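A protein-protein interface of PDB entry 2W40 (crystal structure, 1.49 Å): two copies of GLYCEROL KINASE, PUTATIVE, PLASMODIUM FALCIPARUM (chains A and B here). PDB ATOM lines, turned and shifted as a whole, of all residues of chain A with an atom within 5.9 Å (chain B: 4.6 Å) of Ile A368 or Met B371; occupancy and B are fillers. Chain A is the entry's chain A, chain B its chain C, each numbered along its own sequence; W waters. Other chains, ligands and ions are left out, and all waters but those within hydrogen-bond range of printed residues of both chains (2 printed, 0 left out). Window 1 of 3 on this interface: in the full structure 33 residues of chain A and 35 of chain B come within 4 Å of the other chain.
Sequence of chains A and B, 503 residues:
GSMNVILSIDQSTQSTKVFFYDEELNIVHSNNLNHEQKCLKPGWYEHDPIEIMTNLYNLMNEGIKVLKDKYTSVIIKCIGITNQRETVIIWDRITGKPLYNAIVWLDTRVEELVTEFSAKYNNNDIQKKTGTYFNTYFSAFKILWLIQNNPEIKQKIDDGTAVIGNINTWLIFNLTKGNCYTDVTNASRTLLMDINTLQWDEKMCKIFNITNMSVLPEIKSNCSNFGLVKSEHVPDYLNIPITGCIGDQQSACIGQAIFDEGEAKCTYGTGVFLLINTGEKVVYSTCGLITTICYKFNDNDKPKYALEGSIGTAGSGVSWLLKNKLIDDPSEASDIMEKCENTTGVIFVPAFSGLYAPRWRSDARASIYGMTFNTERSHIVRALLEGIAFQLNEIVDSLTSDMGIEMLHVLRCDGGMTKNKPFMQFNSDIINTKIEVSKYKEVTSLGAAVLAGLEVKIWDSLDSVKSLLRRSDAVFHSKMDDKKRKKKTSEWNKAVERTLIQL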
ATOM      1  N   TRP A 320      -5.506   0.167   3.597  1.00  0.00           N
ATOM      2  CA  TRP A 320      -4.815   0.373   2.358  1.00  0.00           C
ATOM      3  C   TRP A 320      -3.710   1.434   2.458  1.00  0.00           C
ATOM      4  O   TRP A 320      -2.639   1.312   1.885  1.00  0.00           O
ATOM      5  CB  TRP A 320      -5.816   0.697   1.296  1.00  0.00           C
ATOM      6  CG  TRP A 320      -5.247   0.843  -0.097  1.00  0.00           C
ATOM      7  CD1 TRP A 320      -5.142  -0.113  -1.009  1.00  0.00           C
ATOM      8  CD2 TRP A 320      -4.745   2.045  -0.690  1.00  0.00           C
ATOM      9  NE1 TRP A 320      -4.548   0.387  -2.147  1.00  0.00           N
ATOM     10  CE2 TRP A 320      -4.347   1.726  -2.006  1.00  0.00           C
ATOM     11  CE3 TRP A 320      -4.627   3.364  -0.255  1.00  0.00           C
ATOM     12  CZ2 TRP A 320      -3.774   2.704  -2.886  1.00  0.00           C
ATOM     13  CZ3 TRP A 320      -4.068   4.316  -1.124  1.00  0.00           C
ATOM     14  CH2 TRP A 320      -3.643   3.958  -2.417  1.00  0.00           C
ATOM     15  N   LEU A 326       1.371   5.328   3.396  1.00  0.00           N
ATOM     16  CA  LEU A 326       0.870   6.670   3.494  1.00  0.00           C
ATOM     17  C   LEU A 326       0.529   7.115   4.900  1.00  0.00           C
ATOM     18  O   LEU A 326       0.452   8.312   5.209  1.00  0.00           O
ATOM     19  CB  LEU A 326      -0.325   6.843   2.537  1.00  0.00           C
ATOM     20  CG  LEU A 326      -0.101   6.854   1.025  1.00  0.00           C
ATOM     21  CD1 LEU A 326      -1.313   6.571   0.091  1.00  0.00           C
ATOM     22  CD2 LEU A 326       0.671   8.136   0.663  1.00  0.00           C
ATOM     23  N   VAL A 346      -7.204  18.853  -1.715  1.00  0.00           N
ATOM     24  CA  VAL A 346      -7.213  17.478  -2.235  1.00  0.00           C
ATOM     25  C   VAL A 346      -8.556  16.833  -1.851  1.00  0.00           C
ATOM     26  O   VAL A 346      -9.041  16.993  -0.704  1.00  0.00           O
ATOM     27  CB  VAL A 346      -6.039  16.673  -1.623  1.00  0.00           C
ATOM     28  CG1 VAL A 346      -6.130  15.207  -1.936  1.00  0.00           C
ATOM     29  CG2 VAL A 346      -4.711  17.227  -2.109  1.00  0.00           C
ATOM     30  N   ILE A 347      -9.116  16.075  -2.799  1.00  0.00           N
ATOM     31  CA  ILE A 347     -10.272  15.254  -2.574  1.00  0.00           C
ATOM     32  C   ILE A 347      -9.887  13.823  -2.984  1.00  0.00           C
ATOM     33  O   ILE A 347      -9.254  13.596  -3.988  1.00  0.00           O
ATOM     34  CB  ILE A 347     -11.539  15.722  -3.382  1.00  0.00           C
ATOM     35  CG1 ILE A 347     -11.823  17.188  -3.036  1.00  0.00           C
ATOM     36  CG2 ILE A 347     -12.732  14.742  -3.229  1.00  0.00           C
ATOM     37  CD1 ILE A 347     -12.830  17.888  -3.919  1.00  0.00           C
ATOM     38  N   PHE A 348     -10.313  12.901  -2.110  1.00  0.00           N
ATOM     39  CA  PHE A 348     -10.041  11.395  -2.305  1.00  0.00           C
ATOM     40  C   PHE A 348     -11.412  10.742  -2.365  1.00  0.00           C
ATOM     41  O   PHE A 348     -12.111  10.719  -1.326  1.00  0.00           O
ATOM     42  CB  PHE A 348      -9.212  10.897  -1.153  1.00  0.00           C
ATOM     43  CG  PHE A 348      -8.532   9.594  -1.323  1.00  0.00           C
ATOM     44  CD1 PHE A 348      -7.351   9.372  -0.652  1.00  0.00           C
ATOM     45  CD2 PHE A 348      -9.015   8.586  -2.132  1.00  0.00           C
ATOM     46  CE1 PHE A 348      -6.692   8.148  -0.752  1.00  0.00           C
ATOM     47  CE2 PHE A 348      -8.306   7.369  -2.239  1.00  0.00           C
ATOM     48  CZ  PHE A 348      -7.169   7.169  -1.508  1.00  0.00           C
ATOM     49  N   VAL A 349     -11.816  10.261  -3.563  1.00  0.00           N
ATOM     50  CA  VAL A 349     -13.057   9.543  -3.680  1.00  0.00           C
ATOM     51  C   VAL A 349     -12.730   8.062  -3.373  1.00  0.00           C
ATOM     52  O   VAL A 349     -12.003   7.437  -4.209  1.00  0.00           O
ATOM     53  CB  VAL A 349     -13.734   9.749  -5.063  1.00  0.00           C
ATOM     54  CG1 VAL A 349     -15.028   8.939  -5.184  1.00  0.00           C
ATOM     55  CG2 VAL A 349     -13.902  11.228  -5.358  1.00  0.00           C
ATOM     56  N   ALA A 351     -13.224   4.772  -3.422  1.00  0.00           N
ATOM     57  CA  ALA A 351     -14.168   3.912  -4.206  1.00  0.00           C
ATOM     58  C   ALA A 351     -13.322   2.684  -4.688  1.00  0.00           C
ATOM     59  O   ALA A 351     -13.425   2.256  -5.824  1.00  0.00           O
ATOM     60  CB  ALA A 351     -14.752   4.643  -5.361  1.00  0.00           C
ATOM     61  N   PHE A 352     -12.527   2.123  -3.778  1.00  0.00           N
ATOM     62  CA  PHE A 352     -11.624   0.985  -4.122  1.00  0.00           C
ATOM     63  C   PHE A 352     -12.409  -0.196  -4.687  1.00  0.00           C
ATOM     64  O   PHE A 352     -11.898  -0.963  -5.539  1.00  0.00           O
ATOM     65  CB  PHE A 352     -10.801   0.539  -2.931  1.00  0.00           C
ATOM     66  CG  PHE A 352      -9.806   1.530  -2.520  1.00  0.00           C
ATOM     67  CD1 PHE A 352      -8.648   1.700  -3.244  1.00  0.00           C
ATOM     68  CD2 PHE A 352      -9.987   2.328  -1.433  1.00  0.00           C
ATOM     69  CE1 PHE A 352      -7.716   2.628  -2.893  1.00  0.00           C
ATOM     70  CE2 PHE A 352      -9.020   3.279  -1.078  1.00  0.00           C
ATOM     71  CZ  PHE A 352      -7.896   3.423  -1.821  1.00  0.00           C
ATOM     72  N   SER A 353     -13.597  -0.407  -4.122  1.00  0.00           N
ATOM     73  CA  SER A 353     -14.531  -1.464  -4.560  1.00  0.00           C
ATOM     74  C   SER A 353     -15.811  -0.895  -5.158  1.00  0.00           C
ATOM     75  O   SER A 353     -16.898  -1.449  -4.996  1.00  0.00           O
ATOM     76  CB  SER A 353     -14.847  -2.439  -3.430  1.00  0.00           C
ATOM     77  OG  SER A 353     -15.463  -1.868  -2.384  1.00  0.00           O
ATOM     78  N   ALA A 364     -17.013   2.840 -10.637  1.00  0.00           N
ATOM     79  CA  ALA A 364     -16.160   3.753  -9.930  1.00  0.00           C
ATOM     80  C   ALA A 364     -14.876   3.111  -9.358  1.00  0.00           C
ATOM     81  O   ALA A 364     -14.910   1.987  -8.847  1.00  0.00           O
ATOM     82  CB  ALA A 364     -16.948   4.464  -8.804  1.00  0.00           C
ATOM     83  N   ARG A 365     -13.780   3.878  -9.392  1.00  0.00           N
ATOM     84  CA  ARG A 365     -12.511   3.392  -8.781  1.00  0.00           C
ATOM     85  C   ARG A 365     -11.968   4.517  -7.863  1.00  0.00           C
ATOM     86  O   ARG A 365     -12.394   5.698  -8.006  1.00  0.00           O
ATOM     87  CB  ARG A 365     -11.492   3.048  -9.846  1.00  0.00           C
ATOM     88  CG  ARG A 365     -11.960   1.967 -10.797  1.00  0.00           C
ATOM     89  CD  ARG A 365     -11.881   0.609 -10.089  1.00  0.00           C
ATOM     90  NE  ARG A 365     -12.191  -0.441 -11.074  1.00  0.00           N
ATOM     91  CZ  ARG A 365     -13.432  -0.852 -11.370  1.00  0.00           C
ATOM     92  NH1 ARG A 365     -14.491  -0.412 -10.699  1.00  0.00           N
ATOM     93  NH2 ARG A 365     -13.659  -1.778 -12.306  1.00  0.00           N
ATOM     94  N   ALA A 366     -11.101   4.178  -6.943  1.00  0.00           N
ATOM     95  CA  ALA A 366     -10.576   5.128  -6.021  1.00  0.00           C
ATOM     96  C   ALA A 366      -9.695   6.150  -6.792  1.00  0.00           C
ATOM     97  O   ALA A 366      -8.871   5.793  -7.635  1.00  0.00           O
ATOM     98  CB  ALA A 366      -9.847   4.450  -4.918  1.00  0.00           C
ATOM     99  N   SER A 367      -9.878   7.445  -6.482  1.00  0.00           N
ATOM    100  CA  SER A 367      -9.326   8.522  -7.278  1.00  0.00           C
ATOM    101  C   SER A 367      -8.973   9.659  -6.333  1.00  0.00           C
ATOM    102  O   SER A 367      -9.642   9.884  -5.292  1.00  0.00           O
ATOM    103  CB  SER A 367     -10.314   9.038  -8.282  1.00  0.00           C
ATOM    104  OG  SER A 367     -11.003   7.992  -8.927  1.00  0.00           O
ATOM    105  N   ILE A 368      -7.833  10.276  -6.614  1.00  0.00           N
ATOM    106  CA  ILE A 368      -7.304  11.409  -5.823  1.00  0.00           C
ATOM    107  C   ILE A 368      -7.124  12.595  -6.759  1.00  0.00           C
ATOM    108  O   ILE A 368      -6.542  12.467  -7.830  1.00  0.00           O
ATOM    109  CB  ILE A 368      -5.968  11.093  -5.096  1.00  0.00           C
ATOM    110  CG1 ILE A 368      -6.026   9.786  -4.337  1.00  0.00           C
ATOM    111  CG2 ILE A 368      -5.605  12.263  -4.142  1.00  0.00           C
ATOM    112  CD1 ILE A 368      -4.697   9.301  -3.770  1.00  0.00           C
ATOM    113  N   TYR A 369      -7.621  13.776  -6.306  1.00  0.00           N
ATOM    114  CA  TYR A 369      -7.647  14.988  -7.094  1.00  0.00           C
ATOM    115  C   TYR A 369      -6.983  16.110  -6.304  1.00  0.00           C
ATOM    116  O   TYR A 369      -6.995  16.096  -5.044  1.00  0.00           O
ATOM    117  CB  TYR A 369      -9.074  15.444  -7.442  1.00  0.00           C
ATOM    118  CG  TYR A 369      -9.835  14.431  -8.172  1.00  0.00           C
ATOM    119  CD1 TYR A 369      -9.730  14.375  -9.519  1.00  0.00           C
ATOM    120  CD2 TYR A 369     -10.715  13.562  -7.530  1.00  0.00           C
ATOM    121  CE1 TYR A 369     -10.423  13.461 -10.285  1.00  0.00           C
ATOM    122  CE2 TYR A 369     -11.452  12.597  -8.290  1.00  0.00           C
ATOM    123  CZ  TYR A 369     -11.287  12.536  -9.650  1.00  0.00           C
ATOM    124  OH  TYR A 369     -12.005  11.579 -10.364  1.00  0.00           O
ATOM    125  N   GLY A 370      -6.373  17.033  -7.029  1.00  0.00           N
ATOM    126  CA  GLY A 370      -5.993  18.361  -6.485  1.00  0.00           C
ATOM    127  C   GLY A 370      -4.674  18.476  -5.824  1.00  0.00           C
ATOM    128  O   GLY A 370      -4.429  19.462  -5.118  1.00  0.00           O
ATOM    129  N   MET A 371      -3.777  17.567  -6.089  1.00  0.00           N
ATOM    130  CA  MET A 371      -2.500  17.580  -5.454  1.00  0.00           C
ATOM    131  C   MET A 371      -1.467  18.526  -6.088  1.00  0.00           C
ATOM    132  O   MET A 371      -1.446  18.715  -7.329  1.00  0.00           O
ATOM    133  CB  MET A 371      -1.893  16.160  -5.483  1.00  0.00           C
ATOM    134  CG  MET A 371      -2.673  15.127  -4.750  1.00  0.00           C
ATOM    135  SD  MET A 371      -1.891  13.491  -4.698  1.00  0.00           S
ATOM    136  CE  MET A 371      -1.720  12.981  -6.482  1.00  0.00           C
ATOM    137  N   ILE A 380      -3.476  13.576   2.110  1.00  0.00           N
ATOM    138  CA  ILE A 380      -4.104  12.416   1.371  1.00  0.00           C
ATOM    139  C   ILE A 380      -4.898  11.535   2.403  1.00  0.00           C
ATOM    140  O   ILE A 380      -6.040  11.194   2.165  1.00  0.00           O
ATOM    141  CB  ILE A 380      -3.022  11.599   0.614  1.00  0.00           C
ATOM    142  CG1 ILE A 380      -2.339  12.539  -0.493  1.00  0.00           C
ATOM    143  CG2 ILE A 380      -3.707  10.232   0.174  1.00  0.00           C
ATOM    144  CD1 ILE A 380      -1.106  11.967  -1.149  1.00  0.00           C
ATOM    145  N   VAL B 346      -4.394   1.847 -13.505  1.00  0.00           N
ATOM    146  CA  VAL B 346      -4.173   3.133 -12.811  1.00  0.00           C
ATOM    147  C   VAL B 346      -3.501   4.128 -13.765  1.00  0.00           C
ATOM    148  O   VAL B 346      -2.555   3.758 -14.518  1.00  0.00           O
ATOM    149  CB  VAL B 346      -3.328   2.974 -11.517  1.00  0.00           C
ATOM    150  CG1 VAL B 346      -2.926   4.355 -10.862  1.00  0.00           C
ATOM    151  CG2 VAL B 346      -4.160   2.069 -10.503  1.00  0.00           C
ATOM    152  N   ALA B 366      -2.275  17.398  -9.856  1.00  0.00           N
ATOM    153  CA  ALA B 366      -1.900  15.992  -9.987  1.00  0.00           C
ATOM    154  C   ALA B 366      -3.054  15.148  -9.485  1.00  0.00           C
ATOM    155  O   ALA B 366      -3.686  15.434  -8.459  1.00  0.00           O
ATOM    156  CB  ALA B 366      -0.597  15.682  -9.225  1.00  0.00           C
ATOM    157  N   SER B 367      -3.404  14.125 -10.288  1.00  0.00           N
ATOM    158  CA  SER B 367      -4.610  13.306 -10.102  1.00  0.00           C
ATOM    159  C   SER B 367      -4.251  11.840 -10.331  1.00  0.00           C
ATOM    160  O   SER B 367      -3.474  11.515 -11.199  1.00  0.00           O
ATOM    161  CB  SER B 367      -5.628  13.696 -11.150  1.00  0.00           C
ATOM    162  OG  SER B 367      -5.814  15.114 -11.047  1.00  0.00           O
ATOM    163  N   ILE B 368      -4.801  10.945  -9.513  1.00  0.00           N
ATOM    164  CA  ILE B 368      -4.629   9.475  -9.644  1.00  0.00           C
ATOM    165  C   ILE B 368      -5.975   8.831  -9.825  1.00  0.00           C
ATOM    166  O   ILE B 368      -6.919   9.162  -9.078  1.00  0.00           O
ATOM    167  CB  ILE B 368      -3.910   8.837  -8.411  1.00  0.00           C
ATOM    168  CG1 ILE B 368      -2.601   9.518  -8.111  1.00  0.00           C
ATOM    169  CG2 ILE B 368      -3.596   7.339  -8.674  1.00  0.00           C
ATOM    170  CD1 ILE B 368      -1.841   9.092  -6.882  1.00  0.00           C
ATOM    171  N   TYR B 369      -6.100   7.983 -10.854  1.00  0.00           N
ATOM    172  CA  TYR B 369      -7.333   7.309 -11.172  1.00  0.00           C
ATOM    173  C   TYR B 369      -7.164   5.808 -11.212  1.00  0.00           C
ATOM    174  O   TYR B 369      -6.078   5.301 -11.466  1.00  0.00           O
ATOM    175  CB  TYR B 369      -7.806   7.722 -12.577  1.00  0.00           C
ATOM    176  CG  TYR B 369      -7.986   9.183 -12.730  1.00  0.00           C
ATOM    177  CD1 TYR B 369      -9.190   9.767 -12.360  1.00  0.00           C
ATOM    178  CD2 TYR B 369      -6.973  10.023 -13.225  1.00  0.00           C
ATOM    179  CE1 TYR B 369      -9.399  11.154 -12.477  1.00  0.00           C
ATOM    180  CE2 TYR B 369      -7.243  11.427 -13.400  1.00  0.00           C
ATOM    181  CZ  TYR B 369      -8.400  11.953 -12.952  1.00  0.00           C
ATOM    182  OH  TYR B 369      -8.628  13.297 -13.087  1.00  0.00           O
ATOM    183  N   GLY B 370      -8.267   5.090 -10.986  1.00  0.00           N
ATOM    184  CA  GLY B 370      -8.305   3.678 -11.306  1.00  0.00           C
ATOM    185  C   GLY B 370      -7.907   2.712 -10.255  1.00  0.00           C
ATOM    186  O   GLY B 370      -7.799   1.495 -10.540  1.00  0.00           O
ATOM    187  N   MET B 371      -7.708   3.196  -9.021  1.00  0.00           N
ATOM    188  CA  MET B 371      -7.209   2.323  -7.934  1.00  0.00           C
ATOM    189  C   MET B 371      -8.280   1.377  -7.364  1.00  0.00           C
ATOM    190  O   MET B 371      -9.471   1.699  -7.236  1.00  0.00           O
ATOM    191  CB  MET B 371      -6.576   3.165  -6.821  1.00  0.00           C
ATOM    192  CG  MET B 371      -5.525   4.180  -7.269  1.00  0.00           C
ATOM    193  SD  MET B 371      -4.649   4.924  -5.929  1.00  0.00           S
ATOM    194  CE  MET B 371      -5.907   6.038  -5.256  1.00  0.00           C
ATOM    195  N   THR B 372      -7.786   0.186  -7.041  1.00  0.00           N
ATOM    196  CA  THR B 372      -8.495  -0.819  -6.332  1.00  0.00           C
ATOM    197  C   THR B 372      -7.737  -1.255  -5.073  1.00  0.00           C
ATOM    198  O   THR B 372      -6.585  -0.825  -4.841  1.00  0.00           O
ATOM    199  CB  THR B 372      -8.796  -2.053  -7.262  1.00  0.00           C
ATOM    200  OG1 THR B 372      -7.582  -2.677  -7.701  1.00  0.00           O
ATOM    201  CG2 THR B 372      -9.746  -1.623  -8.476  1.00  0.00           C
ATOM    202  N   THR B 375      -4.266  -2.420  -5.802  1.00  0.00           N
ATOM    203  CA  THR B 375      -3.246  -1.405  -6.164  1.00  0.00           C
ATOM    204  C   THR B 375      -2.273  -1.238  -5.009  1.00  0.00           C
ATOM    205  O   THR B 375      -2.656  -1.119  -3.867  1.00  0.00           O
ATOM    206  CB  THR B 375      -3.908  -0.060  -6.500  1.00  0.00           C
ATOM    207  OG1 THR B 375      -4.911  -0.297  -7.508  1.00  0.00           O
ATOM    208  CG2 THR B 375      -2.845   1.049  -6.890  1.00  0.00           C
ATOM    209  N   ILE B 380       1.395   2.766  -8.497  1.00  0.00           N
ATOM    210  CA  ILE B 380       1.300   4.253  -8.488  1.00  0.00           C
ATOM    211  C   ILE B 380       2.575   4.872  -9.038  1.00  0.00           C
ATOM    212  O   ILE B 380       2.536   5.797  -9.817  1.00  0.00           O
ATOM    213  CB  ILE B 380       0.936   4.770  -7.073  1.00  0.00           C
ATOM    214  CG1 ILE B 380      -0.451   4.164  -6.655  1.00  0.00           C
ATOM    215  CG2 ILE B 380       1.102   6.294  -6.963  1.00  0.00           C
ATOM    216  CD1 ILE B 380      -0.846   4.389  -5.125  1.00  0.00           C
HETATM  217  O   HOH W   1     -10.819   6.540 -11.156  1.00  0.00           O
HETATM  218  O   HOH W   2      -7.172  17.052  -9.898  1.00  0.00           O
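Ala A366 touches Met B371, and with the chains exchanged Met A371 touches Ala B366.
Ser A367 touches Ile B368, and with the chains exchanged Ile A368 touches Ser B367.
Ile A368 touches its own counterpart, Ile B368.
Ile A368 touches Met B371, and with the chains exchanged Met A371 touches Ile B368.
Positions printed for both chains: 346, 366, 367, 368, 369, 370, 371 and 380.
The backbone NH (N) of Tyr A369 is in hydrogen-bond range of the backbone carbonyl oxygen (O) of Ile A347 (2.8 Å).
The backbone NH of Val A349 sits at hydrogen-bond distance from the backbone carbonyl oxygen of Ser A367, 2.8 Å away.
O of Ala A351 is in hydrogen-bond range of N of Ala A366, 3.2 Å away.
The backbone carbonyl oxygen of Arg A365 is in hydrogen-bond range of the side-chain hydroxyl of Ser A367, at 2.8 Å.
OG1 of Thr B375 lies within hydrogen-bond range of N of Thr B372 (3.0 Å).
The indole nitrogen (NE1) of Trp A320 is in hydrogen-bond range of the backbone carbonyl oxygen (O) of Thr B375 (3.0 Å).
The backbone NH of Gly B370 lies within hydrogen-bond range of the backbone carbonyl oxygen of Ala A366 (3.5 Å).
The backbone NH (N) of Ala A366 is in hydrogen-bond range of the backbone carbonyl oxygen (O) of Met B371, 3.0 Å away.
The backbone NH of Ile A368 lies within hydrogen-bond range of the backbone carbonyl oxygen of Ile B368 (2.9 Å).
The backbone NH of Gly A370 is in hydrogen-bond range of the backbone carbonyl oxygen of Ala B366, at 3.4 Å.
O of Met A371 is in hydrogen-bond range of N of Ala B366.
Trp A320 touches Thr B372 (NE1 to O, 3.6 Å).
Ile B380 touches Trp A320.
O of Met B371 touches CA of Phe A352, 3.9 Å away.
Phe A352 touches Thr B372.
Gly B370 touches Arg A365 (CA to CB, 3.6 Å).
CA of Ser A367 touches O of Ile B368, at 3.1 Å.
CE of Met B371 touches CD1 of Ile A368 (3.8 Å).
Ala B366 touches Tyr A369 (O to C, 3.996 Å).
Tyr B369 touches Tyr A369 (OH to CE1, 3.3 Å).
Met A371 touches Ile B368.
Of the 18 printed residues of chain A, 9 touch a printed residue of chain B.
Along chain A the printed residues that touch a printed residue of chain B span positions 320 to 371.
Among the printed residues, 21 pairs touch across the chains.
Water W2 bridges OG of Ser B367 (2.6 Å) and N of Gly A370 (3.0 Å).
Water W1 bridges the side-chain hydroxyl (OG) of Ser A367 (2.7 Å) and the backbone NH (N) of Gly B370 (2.9 Å).
Leu A326 touches none of the printed residues of chain B.
Phe A348 touches none of the printed residues of chain B.
Of chain B, only Ser B367 (3.1 Å), Ile B368 (2.9 Å) and Met B371 (3.8 Å) come within 4 Å of Ile A368.
Of the printed residues of chain A, Tyr B369 touches Ala A366 and Tyr A369.
Met B371 touches five residues of chain A.
Of the printed residues of chain A, Thr B375 touches Trp A320 (3.0 Å).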
